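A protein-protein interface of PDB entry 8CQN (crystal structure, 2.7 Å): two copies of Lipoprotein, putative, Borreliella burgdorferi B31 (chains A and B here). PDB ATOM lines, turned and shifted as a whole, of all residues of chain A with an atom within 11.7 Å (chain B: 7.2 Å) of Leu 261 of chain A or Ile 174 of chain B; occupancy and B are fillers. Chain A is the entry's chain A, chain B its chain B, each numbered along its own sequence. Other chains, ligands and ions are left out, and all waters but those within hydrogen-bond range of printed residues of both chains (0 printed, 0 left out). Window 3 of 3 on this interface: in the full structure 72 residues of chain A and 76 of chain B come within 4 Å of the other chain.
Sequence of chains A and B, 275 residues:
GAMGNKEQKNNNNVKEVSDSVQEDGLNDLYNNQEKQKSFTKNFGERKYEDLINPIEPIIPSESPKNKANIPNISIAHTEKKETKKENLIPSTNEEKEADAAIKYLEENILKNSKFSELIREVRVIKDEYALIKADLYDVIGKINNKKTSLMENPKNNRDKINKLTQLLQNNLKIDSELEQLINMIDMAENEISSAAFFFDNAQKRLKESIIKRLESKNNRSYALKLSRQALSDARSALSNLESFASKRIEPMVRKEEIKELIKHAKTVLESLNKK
The side-chain carboxylate of Glu 177 of chain B is in salt-bridge range of the guanidinium group of Arg 254 of chain A, 3.2 Å away.
NZ of Lys 259 of chain A is in salt-bridge range of OE2 of Glu 256 of chain A (3.5 Å). NZ of Lys 255 of chain A lies within salt-bridge range of OE1 of Glu 256 of chain A.
Among the printed residues, pairs that only touch across the chains: Pro 251 of chain A with Leu 181 of chain B, Arg 254 of chain A with Leu 181 of chain B, Lys 255 of chain A with Ile 132 of chain B, Ile 258 of chain A with Ile 132 of chain B, Ile 258 of chain A with Ile 174 of chain B, Ile 258 of chain A with Leu 181 of chain B, Lys 259 of chain A with Ile 132 of chain B, Leu 261 of chain A with Ile 174 of chain B and Ile 262 of chain A with Ile 132 of chain B.
Printed residues of chain B within 4 Å of Pro 251 of chain A: Leu 181. Of the printed residues of chain B, Arg 254 of chain A touches Glu 177 and Leu 181. Printed residues of chain B within 4 Å of Lys 259 of chain A: Ile 132. Of the printed residues of chain B, Leu 261 of chain A touches Ile 174 (3.5 Å). No residue of chain A comes within 4 Å of Asn 171 of chain B. No residue of chain A comes within 4 Å of Lys 173 of chain B. Of the printed residues of chain A, Ile 174 of chain B touches Ile 258 and Leu 261. No residue of chain A comes within 4 Å of Ser 176 of chain B. No residue of chain A comes within 4 Å of Leu 178 of chain B.
Of the 18 printed residues of chain A, 7 touch a printed residue of chain B. Of the 18 printed residues of chain B, 4 touch a printed residue of chain A. Printed residues of chain B that touch a printed residue of chain A: Ile 132, Ile 174, Glu 177 and Leu 181. Hydrophobic or aromatic side chains of chain B within 4 Å of the printed part of chain A: Ile 132, Ile 174 and Leu 181.
No position is printed for both chains.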
ATOM      1  N   PRO A 251     -27.582   6.727 -16.151  1.00  0.00           N
ATOM      2  CA  PRO A 251     -27.814   6.000 -17.397  1.00  0.00           C
ATOM      3  C   PRO A 251     -28.338   6.930 -18.505  1.00  0.00           C
ATOM      4  O   PRO A 251     -27.848   6.833 -19.606  1.00  0.00           O
ATOM      5  CB  PRO A 251     -28.835   4.948 -16.964  1.00  0.00           C
ATOM      6  CG  PRO A 251     -28.526   4.754 -15.517  1.00  0.00           C
ATOM      7  CD  PRO A 251     -28.275   6.149 -14.992  1.00  0.00           C
ATOM      8  N   VAL A 253     -27.737   9.976 -18.932  1.00  0.00           N
ATOM      9  CA  VAL A 253     -26.727  11.048 -19.180  1.00  0.00           C
ATOM     10  C   VAL A 253     -25.461  10.482 -19.858  1.00  0.00           C
ATOM     11  O   VAL A 253     -24.762  11.244 -20.576  1.00  0.00           O
ATOM     12  CB  VAL A 253     -26.445  11.742 -17.838  1.00  0.00           C
ATOM     13  CG1 VAL A 253     -24.968  11.912 -17.508  1.00  0.00           C
ATOM     14  CG2 VAL A 253     -27.197  13.054 -17.764  1.00  0.00           C
ATOM     15  N   ARG A 254     -25.129   9.214 -19.647  1.00  0.00           N
ATOM     16  CA  ARG A 254     -23.871   8.664 -20.187  1.00  0.00           C
ATOM     17  C   ARG A 254     -24.121   7.844 -21.452  1.00  0.00           C
ATOM     18  O   ARG A 254     -23.132   7.350 -21.988  1.00  0.00           O
ATOM     19  CB  ARG A 254     -23.190   7.810 -19.126  1.00  0.00           C
ATOM     20  CG  ARG A 254     -23.076   8.520 -17.794  1.00  0.00           C
ATOM     21  CD  ARG A 254     -22.845   7.491 -16.718  1.00  0.00           C
ATOM     22  NE  ARG A 254     -22.560   8.085 -15.417  1.00  0.00           N
ATOM     23  CZ  ARG A 254     -22.011   7.430 -14.393  1.00  0.00           C
ATOM     24  NH1 ARG A 254     -21.698   6.148 -14.511  1.00  0.00           N
ATOM     25  NH2 ARG A 254     -21.776   8.062 -13.252  1.00  0.00           N
ATOM     26  N   LYS A 255     -25.367   7.715 -21.915  1.00  0.00           N
ATOM     27  CA  LYS A 255     -25.759   6.801 -23.025  1.00  0.00           C
ATOM     28  C   LYS A 255     -25.042   7.233 -24.303  1.00  0.00           C
ATOM     29  O   LYS A 255     -24.098   6.515 -24.747  1.00  0.00           O
ATOM     30  CB  LYS A 255     -27.281   6.778 -23.210  1.00  0.00           C
ATOM     31  CG  LYS A 255     -27.808   5.922 -24.356  1.00  0.00           C
ATOM     32  CD  LYS A 255     -29.306   5.991 -24.500  1.00  0.00           C
ATOM     33  CE  LYS A 255     -29.759   7.245 -25.215  1.00  0.00           C
ATOM     34  NZ  LYS A 255     -31.231   7.407 -25.155  1.00  0.00           N
ATOM     35  N   GLU A 256     -25.408   8.389 -24.840  1.00  0.00           N
ATOM     36  CA  GLU A 256     -24.782   8.930 -26.074  1.00  0.00           C
ATOM     37  C   GLU A 256     -23.274   9.089 -25.840  1.00  0.00           C
ATOM     38  O   GLU A 256     -22.537   8.840 -26.795  1.00  0.00           O
ATOM     39  CB  GLU A 256     -25.462  10.212 -26.559  1.00  0.00           C
ATOM     40  CG  GLU A 256     -26.201  10.010 -27.871  1.00  0.00           C
ATOM     41  CD  GLU A 256     -27.531   9.306 -27.714  1.00  0.00           C
ATOM     42  OE1 GLU A 256     -28.017   9.261 -26.577  1.00  0.00           O
ATOM     43  OE2 GLU A 256     -28.076   8.804 -28.721  1.00  0.00           O
ATOM     44  N   GLU A 257     -22.814   9.448 -24.637  1.00  0.00           N
ATOM     45  CA  GLU A 257     -21.348   9.571 -24.377  1.00  0.00           C
ATOM     46  C   GLU A 257     -20.733   8.205 -24.667  1.00  0.00           C
ATOM     47  O   GLU A 257     -19.555   8.134 -25.067  1.00  0.00           O
ATOM     48  CB  GLU A 257     -20.963   9.960 -22.945  1.00  0.00           C
ATOM     49  CG  GLU A 257     -21.756  11.117 -22.373  1.00  0.00           C
ATOM     50  CD  GLU A 257     -21.433  12.488 -22.932  1.00  0.00           C
ATOM     51  OE1 GLU A 257     -20.239  12.852 -22.955  1.00  0.00           O
ATOM     52  OE2 GLU A 257     -22.390  13.192 -23.327  1.00  0.00           O
ATOM     53  N   ILE A 258     -21.513   7.147 -24.472  1.00  0.00           N
ATOM     54  CA  ILE A 258     -20.991   5.765 -24.598  1.00  0.00           C
ATOM     55  C   ILE A 258     -21.189   5.289 -26.028  1.00  0.00           C
ATOM     56  O   ILE A 258     -20.271   4.617 -26.505  1.00  0.00           O
ATOM     57  CB  ILE A 258     -21.603   4.833 -23.542  1.00  0.00           C
ATOM     58  CG1 ILE A 258     -20.993   5.176 -22.181  1.00  0.00           C
ATOM     59  CG2 ILE A 258     -21.385   3.362 -23.925  1.00  0.00           C
ATOM     60  CD1 ILE A 258     -21.706   4.581 -21.002  1.00  0.00           C
ATOM     61  N   LYS A 259     -22.318   5.642 -26.651  1.00  0.00           N
ATOM     62  CA  LYS A 259     -22.582   5.384 -28.086  1.00  0.00           C
ATOM     63  C   LYS A 259     -21.383   5.893 -28.906  1.00  0.00           C
ATOM     64  O   LYS A 259     -20.821   5.089 -29.689  1.00  0.00           O
ATOM     65  CB  LYS A 259     -23.908   6.007 -28.532  1.00  0.00           C
ATOM     66  CG  LYS A 259     -25.161   5.197 -28.178  1.00  0.00           C
ATOM     67  CD  LYS A 259     -26.143   5.010 -29.330  1.00  0.00           C
ATOM     68  CE  LYS A 259     -27.310   5.973 -29.332  1.00  0.00           C
ATOM     69  NZ  LYS A 259     -28.519   5.373 -28.714  1.00  0.00           N
ATOM     70  N   GLU A 260     -20.962   7.145 -28.712  1.00  0.00           N
ATOM     71  CA  GLU A 260     -19.822   7.729 -29.469  1.00  0.00           C
ATOM     72  C   GLU A 260     -18.534   7.005 -29.057  1.00  0.00           C
ATOM     73  O   GLU A 260     -17.750   6.653 -29.955  1.00  0.00           O
ATOM     74  CB  GLU A 260     -19.707   9.251 -29.316  1.00  0.00           C
ATOM     75  CG  GLU A 260     -20.091   9.778 -27.943  1.00  0.00           C
ATOM     76  CD  GLU A 260     -19.455  11.101 -27.530  1.00  0.00           C
ATOM     77  OE1 GLU A 260     -18.216  11.229 -27.679  1.00  0.00           O
ATOM     78  OE2 GLU A 260     -20.200  12.004 -27.045  1.00  0.00           O
ATOM     79  N   LEU A 261     -18.326   6.760 -27.763  1.00  0.00           N
ATOM     80  CA  LEU A 261     -17.074   6.142 -27.241  1.00  0.00           C
ATOM     81  C   LEU A 261     -16.877   4.775 -27.902  1.00  0.00           C
ATOM     82  O   LEU A 261     -15.735   4.433 -28.225  1.00  0.00           O
ATOM     83  CB  LEU A 261     -17.161   6.018 -25.719  1.00  0.00           C
ATOM     84  CG  LEU A 261     -15.895   5.557 -24.996  1.00  0.00           C
ATOM     85  CD1 LEU A 261     -14.977   6.728 -24.646  1.00  0.00           C
ATOM     86  CD2 LEU A 261     -16.254   4.801 -23.733  1.00  0.00           C
ATOM     87  N   ILE A 262     -17.949   4.021 -28.120  1.00  0.00           N
ATOM     88  CA  ILE A 262     -17.882   2.794 -28.966  1.00  0.00           C
ATOM     89  C   ILE A 262     -17.458   3.240 -30.369  1.00  0.00           C
ATOM     90  O   ILE A 262     -16.314   2.955 -30.758  1.00  0.00           O
ATOM     91  CB  ILE A 262     -19.218   2.016 -28.997  1.00  0.00           C
ATOM     92  CG1 ILE A 262     -19.664   1.532 -27.615  1.00  0.00           C
ATOM     93  CG2 ILE A 262     -19.117   0.849 -29.969  1.00  0.00           C
ATOM     94  CD1 ILE A 262     -21.076   0.959 -27.599  1.00  0.00           C
ATOM     95  N   LYS A 263     -18.346   3.971 -31.058  1.00  0.00           N
ATOM     96  CA  LYS A 263     -18.353   4.161 -32.539  1.00  0.00           C
ATOM     97  C   LYS A 263     -17.394   5.286 -32.940  1.00  0.00           C
ATOM     98  O   LYS A 263     -17.388   5.665 -34.132  1.00  0.00           O
ATOM     99  CB  LYS A 263     -19.764   4.447 -33.072  1.00  0.00           C
ATOM    100  CG  LYS A 263     -20.744   3.279 -33.013  1.00  0.00           C
ATOM    101  CD  LYS A 263     -22.062   3.536 -33.737  1.00  0.00           C
ATOM    102  CE  LYS A 263     -23.267   2.921 -33.054  1.00  0.00           C
ATOM    103  NZ  LYS A 263     -23.397   3.373 -31.646  1.00  0.00           N
ATOM    104  N   HIS A 264     -16.612   5.798 -31.992  1.00  0.00           N
ATOM    105  CA  HIS A 264     -15.293   6.400 -32.297  1.00  0.00           C
ATOM    106  C   HIS A 264     -14.347   5.262 -32.687  1.00  0.00           C
ATOM    107  O   HIS A 264     -13.761   5.344 -33.780  1.00  0.00           O
ATOM    108  CB  HIS A 264     -14.730   7.204 -31.124  1.00  0.00           C
ATOM    109  CG  HIS A 264     -13.366   7.728 -31.417  1.00  0.00           C
ATOM    110  ND1 HIS A 264     -12.231   6.993 -31.151  1.00  0.00           N
ATOM    111  CD2 HIS A 264     -12.959   8.876 -32.004  1.00  0.00           C
ATOM    112  CE1 HIS A 264     -11.173   7.679 -31.535  1.00  0.00           C
ATOM    113  NE2 HIS A 264     -11.594   8.841 -32.062  1.00  0.00           N
ATOM    114  N   ALA A 265     -14.241   4.231 -31.836  1.00  0.00           N
ATOM    115  CA  ALA A 265     -13.232   3.141 -31.910  1.00  0.00           C
ATOM    116  C   ALA A 265     -13.620   2.050 -32.931  1.00  0.00           C
ATOM    117  O   ALA A 265     -12.781   1.143 -33.165  1.00  0.00           O
ATOM    118  CB  ALA A 265     -13.017   2.554 -30.534  1.00  0.00           C
ATOM    119  N   LYS A 266     -14.826   2.118 -33.514  1.00  0.00           N
ATOM    120  CA  LYS A 266     -15.252   1.268 -34.667  1.00  0.00           C
ATOM    121  C   LYS A 266     -14.419   1.662 -35.903  1.00  0.00           C
ATOM    122  O   LYS A 266     -13.819   0.757 -36.518  1.00  0.00           O
ATOM    123  CB  LYS A 266     -16.761   1.401 -34.940  1.00  0.00           C
ATOM    124  CG  LYS A 266     -17.514   0.101 -35.210  1.00  0.00           C
ATOM    125  CD  LYS A 266     -19.026   0.175 -34.981  1.00  0.00           C
ATOM    126  CE  LYS A 266     -19.580  -1.029 -34.238  1.00  0.00           C
ATOM    127  NZ  LYS A 266     -21.001  -0.867 -33.849  1.00  0.00           N
ATOM    128  N   THR A 267     -14.361   2.961 -36.241  1.00  0.00           N
ATOM    129  CA  THR A 267     -13.622   3.528 -37.413  1.00  0.00           C
ATOM    130  C   THR A 267     -12.099   3.314 -37.253  1.00  0.00           C
ATOM    131  O   THR A 267     -11.382   3.322 -38.288  1.00  0.00           O
ATOM    132  CB  THR A 267     -13.954   5.016 -37.609  1.00  0.00           C
ATOM    133  OG1 THR A 267     -13.539   5.679 -36.413  1.00  0.00           O
ATOM    134  CG2 THR A 267     -15.417   5.303 -37.873  1.00  0.00           C
ATOM    135  N   VAL A 268     -11.602   3.128 -36.020  1.00  0.00           N
ATOM    136  CA  VAL A 268     -10.164   2.822 -35.740  1.00  0.00           C
ATOM    137  C   VAL A 268      -9.923   1.305 -35.934  1.00  0.00           C
ATOM    138  O   VAL A 268      -8.744   0.924 -36.165  1.00  0.00           O
ATOM    139  CB  VAL A 268      -9.724   3.329 -34.349  1.00  0.00           C
ATOM    140  CG1 VAL A 268      -8.208   3.359 -34.198  1.00  0.00           C
ATOM    141  CG2 VAL A 268     -10.288   4.707 -34.034  1.00  0.00           C
ATOM    142  N   LEU A 269     -10.976   0.467 -35.873  1.00  0.00           N
ATOM    143  CA  LEU A 269     -10.942  -0.948 -36.362  1.00  0.00           C
ATOM    144  C   LEU A 269     -10.955  -0.955 -37.902  1.00  0.00           C
ATOM    145  O   LEU A 269     -10.188  -1.749 -38.498  1.00  0.00           O
ATOM    146  CB  LEU A 269     -12.128  -1.769 -35.828  1.00  0.00           C
ATOM    147  CG  LEU A 269     -11.928  -2.601 -34.553  1.00  0.00           C
ATOM    148  CD1 LEU A 269     -12.476  -4.017 -34.747  1.00  0.00           C
ATOM    149  CD2 LEU A 269     -10.474  -2.657 -34.093  1.00  0.00           C
ATOM    150  N   ILE B 132     -26.485  -1.397 -26.981  1.00  0.00           N
ATOM    151  CA  ILE B 132     -25.121  -0.854 -26.739  1.00  0.00           C
ATOM    152  C   ILE B 132     -24.188  -1.941 -26.193  1.00  0.00           C
ATOM    153  O   ILE B 132     -23.062  -1.955 -26.641  1.00  0.00           O
ATOM    154  CB  ILE B 132     -25.232   0.387 -25.830  1.00  0.00           C
ATOM    155  CG1 ILE B 132     -25.635   1.607 -26.662  1.00  0.00           C
ATOM    156  CG2 ILE B 132     -23.971   0.632 -25.021  1.00  0.00           C
ATOM    157  CD1 ILE B 132     -26.124   2.782 -25.848  1.00  0.00           C
ATOM    158  N   LEU B 136     -20.830  -3.316 -28.101  1.00  0.00           N
ATOM    159  CA  LEU B 136     -19.528  -3.446 -27.400  1.00  0.00           C
ATOM    160  C   LEU B 136     -19.017  -4.886 -27.553  1.00  0.00           C
ATOM    161  O   LEU B 136     -17.919  -5.035 -28.105  1.00  0.00           O
ATOM    162  CB  LEU B 136     -19.678  -3.073 -25.923  1.00  0.00           C
ATOM    163  CG  LEU B 136     -18.360  -3.046 -25.146  1.00  0.00           C
ATOM    164  CD1 LEU B 136     -17.476  -1.905 -25.640  1.00  0.00           C
ATOM    165  CD2 LEU B 136     -18.589  -2.933 -23.646  1.00  0.00           C
ATOM    166  N   ILE B 140     -15.652  -6.152 -29.357  1.00  0.00           N
ATOM    167  CA  ILE B 140     -14.641  -6.876 -28.532  1.00  0.00           C
ATOM    168  C   ILE B 140     -14.141  -8.065 -29.360  1.00  0.00           C
ATOM    169  O   ILE B 140     -12.933  -8.127 -29.617  1.00  0.00           O
ATOM    170  CB  ILE B 140     -15.212  -7.311 -27.167  1.00  0.00           C
ATOM    171  CG1 ILE B 140     -15.370  -6.114 -26.225  1.00  0.00           C
ATOM    172  CG2 ILE B 140     -14.370  -8.417 -26.542  1.00  0.00           C
ATOM    173  CD1 ILE B 140     -14.107  -5.305 -26.020  1.00  0.00           C
ATOM    174  N   LEU B 167      -7.014  -1.022 -25.665  1.00  0.00           N
ATOM    175  CA  LEU B 167      -8.431  -0.904 -26.119  1.00  0.00           C
ATOM    176  C   LEU B 167      -9.288  -1.957 -25.416  1.00  0.00           C
ATOM    177  O   LEU B 167     -10.227  -1.550 -24.714  1.00  0.00           O
ATOM    178  CB  LEU B 167      -8.557  -1.065 -27.640  1.00  0.00           C
ATOM    179  CG  LEU B 167      -8.875   0.211 -28.419  1.00  0.00           C
ATOM    180  CD1 LEU B 167      -9.706  -0.102 -29.663  1.00  0.00           C
ATOM    181  CD2 LEU B 167      -9.577   1.237 -27.542  1.00  0.00           C
ATOM    182  N   LEU B 168      -8.977  -3.244 -25.618  1.00  0.00           N
ATOM    183  CA  LEU B 168      -9.635  -4.402 -24.941  1.00  0.00           C
ATOM    184  C   LEU B 168      -9.874  -4.058 -23.461  1.00  0.00           C
ATOM    185  O   LEU B 168     -11.047  -4.099 -23.031  1.00  0.00           O
ATOM    186  CB  LEU B 168      -8.757  -5.651 -25.117  1.00  0.00           C
ATOM    187  CG  LEU B 168      -9.108  -6.870 -24.258  1.00  0.00           C
ATOM    188  CD1 LEU B 168      -9.112  -8.142 -25.100  1.00  0.00           C
ATOM    189  CD2 LEU B 168      -8.157  -7.008 -23.071  1.00  0.00           C
ATOM    190  N   GLN B 169      -8.807  -3.697 -22.736  1.00  0.00           N
ATOM    191  CA  GLN B 169      -8.858  -3.223 -21.325  1.00  0.00           C
ATOM    192  C   GLN B 169      -9.629  -1.893 -21.241  1.00  0.00           C
ATOM    193  O   GLN B 169     -10.526  -1.808 -20.382  1.00  0.00           O
ATOM    194  CB  GLN B 169      -7.448  -3.091 -20.742  1.00  0.00           C
ATOM    195  CG  GLN B 169      -6.792  -4.428 -20.403  1.00  0.00           C
ATOM    196  CD  GLN B 169      -5.579  -4.273 -19.514  1.00  0.00           C
ATOM    197  OE1 GLN B 169      -5.268  -3.183 -19.031  1.00  0.00           O
ATOM    198  NE2 GLN B 169      -4.897  -5.378 -19.260  1.00  0.00           N
ATOM    199  N   ASN B 170      -9.316  -0.912 -22.106  1.00  0.00           N
ATOM    200  CA  ASN B 170     -10.003   0.414 -22.197  1.00  0.00           C
ATOM    201  C   ASN B 170     -11.493   0.212 -22.526  1.00  0.00           C
ATOM    202  O   ASN B 170     -12.302   1.112 -22.222  1.00  0.00           O
ATOM    203  CB  ASN B 170      -9.363   1.354 -23.235  1.00  0.00           C
ATOM    204  CG  ASN B 170      -8.726   2.595 -22.639  1.00  0.00           C
ATOM    205  OD1 ASN B 170      -7.976   2.506 -21.674  1.00  0.00           O
ATOM    206  ND2 ASN B 170      -9.000   3.752 -23.220  1.00  0.00           N
ATOM    207  N   ASN B 171     -11.848  -0.914 -23.151  1.00  0.00           N
ATOM    208  CA  ASN B 171     -13.237  -1.211 -23.591  1.00  0.00           C
ATOM    209  C   ASN B 171     -13.790  -2.412 -22.818  1.00  0.00           C
ATOM    210  O   ASN B 171     -14.894  -2.862 -23.163  1.00  0.00           O
ATOM    211  CB  ASN B 171     -13.315  -1.368 -25.112  1.00  0.00           C
ATOM    212  CG  ASN B 171     -13.229  -0.025 -25.804  1.00  0.00           C
ATOM    213  OD1 ASN B 171     -13.389   1.011 -25.154  1.00  0.00           O
ATOM    214  ND2 ASN B 171     -12.982  -0.027 -27.105  1.00  0.00           N
ATOM    215  N   LEU B 172     -13.079  -2.888 -21.793  1.00  0.00           N
ATOM    216  CA  LEU B 172     -13.640  -3.849 -20.810  1.00  0.00           C
ATOM    217  C   LEU B 172     -14.037  -3.095 -19.535  1.00  0.00           C
ATOM    218  O   LEU B 172     -15.078  -3.472 -18.957  1.00  0.00           O
ATOM    219  CB  LEU B 172     -12.643  -4.977 -20.526  1.00  0.00           C
ATOM    220  CG  LEU B 172     -12.787  -6.244 -21.376  1.00  0.00           C
ATOM    221  CD1 LEU B 172     -12.596  -7.482 -20.513  1.00  0.00           C
ATOM    222  CD2 LEU B 172     -14.127  -6.318 -22.105  1.00  0.00           C
ATOM    223  N   LYS B 173     -13.286  -2.067 -19.119  1.00  0.00           N
ATOM    224  CA  LYS B 173     -13.627  -1.311 -17.884  1.00  0.00           C
ATOM    225  C   LYS B 173     -15.003  -0.686 -18.097  1.00  0.00           C
ATOM    226  O   LYS B 173     -15.851  -0.745 -17.164  1.00  0.00           O
ATOM    227  CB  LYS B 173     -12.600  -0.233 -17.524  1.00  0.00           C
ATOM    228  CG  LYS B 173     -12.626   0.169 -16.051  1.00  0.00           C
ATOM    229  CD  LYS B 173     -12.054   1.533 -15.763  1.00  0.00           C
ATOM    230  CE  LYS B 173     -11.461   1.634 -14.373  1.00  0.00           C
ATOM    231  NZ  LYS B 173     -11.326   3.043 -13.939  1.00  0.00           N
ATOM    232  N   ILE B 174     -15.199  -0.127 -19.293  1.00  0.00           N
ATOM    233  CA  ILE B 174     -16.528   0.349 -19.757  1.00  0.00           C
ATOM    234  C   ILE B 174     -17.520  -0.806 -19.636  1.00  0.00           C
ATOM    235  O   ILE B 174     -18.587  -0.589 -19.024  1.00  0.00           O
ATOM    236  CB  ILE B 174     -16.512   0.899 -21.188  1.00  0.00           C
ATOM    237  CG1 ILE B 174     -17.929   0.903 -21.760  1.00  0.00           C
ATOM    238  CG2 ILE B 174     -15.581   0.120 -22.078  1.00  0.00           C
ATOM    239  CD1 ILE B 174     -18.123   1.922 -22.828  1.00  0.00           C
ATOM    240  N   ASP B 175     -17.190  -1.979 -20.182  1.00  0.00           N
ATOM    241  CA  ASP B 175     -18.106  -3.152 -20.132  1.00  0.00           C
ATOM    242  C   ASP B 175     -18.588  -3.270 -18.680  1.00  0.00           C
ATOM    243  O   ASP B 175     -19.787  -3.545 -18.481  1.00  0.00           O
ATOM    244  CB  ASP B 175     -17.494  -4.443 -20.712  1.00  0.00           C
ATOM    245  CG  ASP B 175     -18.506  -5.568 -20.953  1.00  0.00           C
ATOM    246  OD1 ASP B 175     -19.183  -5.578 -22.011  1.00  0.00           O
ATOM    247  OD2 ASP B 175     -18.630  -6.435 -20.073  1.00  0.00           O
ATOM    248  N   SER B 176     -17.722  -2.989 -17.702  1.00  0.00           N
ATOM    249  CA  SER B 176     -18.132  -2.931 -16.277  1.00  0.00           C
ATOM    250  C   SER B 176     -19.035  -1.722 -16.037  1.00  0.00           C
ATOM    251  O   SER B 176     -20.231  -1.950 -15.732  1.00  0.00           O
ATOM    252  CB  SER B 176     -16.984  -2.954 -15.335  1.00  0.00           C
ATOM    253  OG  SER B 176     -17.217  -3.992 -14.400  1.00  0.00           O
ATOM    254  N   GLU B 177     -18.514  -0.498 -16.183  1.00  0.00           N
ATOM    255  CA  GLU B 177     -19.303   0.739 -15.909  1.00  0.00           C
ATOM    256  C   GLU B 177     -20.682   0.539 -16.528  1.00  0.00           C
ATOM    257  O   GLU B 177     -21.691   0.901 -15.881  1.00  0.00           O
ATOM    258  CB  GLU B 177     -18.643   1.991 -16.471  1.00  0.00           C
ATOM    259  CG  GLU B 177     -19.565   3.199 -16.502  1.00  0.00           C
ATOM    260  CD  GLU B 177     -18.869   4.521 -16.780  1.00  0.00           C
ATOM    261  OE1 GLU B 177     -19.551   5.559 -16.842  1.00  0.00           O
ATOM    262  OE2 GLU B 177     -17.640   4.509 -16.937  1.00  0.00           O
ATOM    263  N   LEU B 178     -20.700  -0.090 -17.705  1.00  0.00           N
ATOM    264  CA  LEU B 178     -21.933  -0.435 -18.445  1.00  0.00           C
ATOM    265  C   LEU B 178     -22.820  -1.346 -17.591  1.00  0.00           C
ATOM    266  O   LEU B 178     -24.007  -1.034 -17.493  1.00  0.00           O
ATOM    267  CB  LEU B 178     -21.548  -1.110 -19.764  1.00  0.00           C
ATOM    268  CG  LEU B 178     -22.611  -1.080 -20.863  1.00  0.00           C
ATOM    269  CD1 LEU B 178     -22.934   0.348 -21.271  1.00  0.00           C
ATOM    270  CD2 LEU B 178     -22.161  -1.874 -22.085  1.00  0.00           C
ATOM    271  N   GLU B 179     -22.277  -2.433 -17.022  1.00  0.00           N
ATOM    272  CA  GLU B 179     -23.054  -3.442 -16.234  1.00  0.00           C
ATOM    273  C   GLU B 179     -23.722  -2.734 -15.045  1.00  0.00           C
ATOM    274  O   GLU B 179     -24.924  -3.031 -14.773  1.00  0.00           O
ATOM    275  CB  GLU B 179     -22.175  -4.608 -15.762  1.00  0.00           C
ATOM    276  CG  GLU B 179     -21.621  -5.474 -16.889  1.00  0.00           C
ATOM    277  CD  GLU B 179     -22.463  -6.631 -17.414  1.00  0.00           C
ATOM    278  OE1 GLU B 179     -22.995  -7.388 -16.578  1.00  0.00           O
ATOM    279  OE2 GLU B 179     -22.550  -6.799 -18.666  1.00  0.00           O
ATOM    280  N   GLN B 180     -22.970  -1.837 -14.388  1.00  0.00           N
ATOM    281  CA  GLN B 180     -23.445  -0.949 -13.299  1.00  0.00           C
ATOM    282  C   GLN B 180     -24.688  -0.190 -13.787  1.00  0.00           C
ATOM    283  O   GLN B 180     -25.783  -0.348 -13.198  1.00  0.00           O
ATOM    284  CB  GLN B 180     -22.329   0.008 -12.870  1.00  0.00           C
ATOM    285  CG  GLN B 180     -21.334  -0.598 -11.884  1.00  0.00           C
ATOM    286  CD  GLN B 180     -20.406   0.424 -11.259  1.00  0.00           C
ATOM    287  OE1 GLN B 180     -19.954   1.378 -11.904  1.00  0.00           O
ATOM    288  NE2 GLN B 180     -20.111   0.221  -9.982  1.00  0.00           N
ATOM    289  N   LEU B 181     -24.526   0.601 -14.839  1.00  0.00           N
ATOM    290  CA  LEU B 181     -25.617   1.411 -15.428  1.00  0.00           C
ATOM    291  C   LEU B 181     -26.811   0.502 -15.738  1.00  0.00           C
ATOM    292  O   LEU B 181     -27.945   0.895 -15.447  1.00  0.00           O
ATOM    293  CB  LEU B 181     -25.131   2.125 -16.691  1.00  0.00           C
ATOM    294  CG  LEU B 181     -23.955   3.086 -16.535  1.00  0.00           C
ATOM    295  CD1 LEU B 181     -23.609   3.718 -17.882  1.00  0.00           C
ATOM    296  CD2 LEU B 181     -24.249   4.153 -15.513  1.00  0.00           C
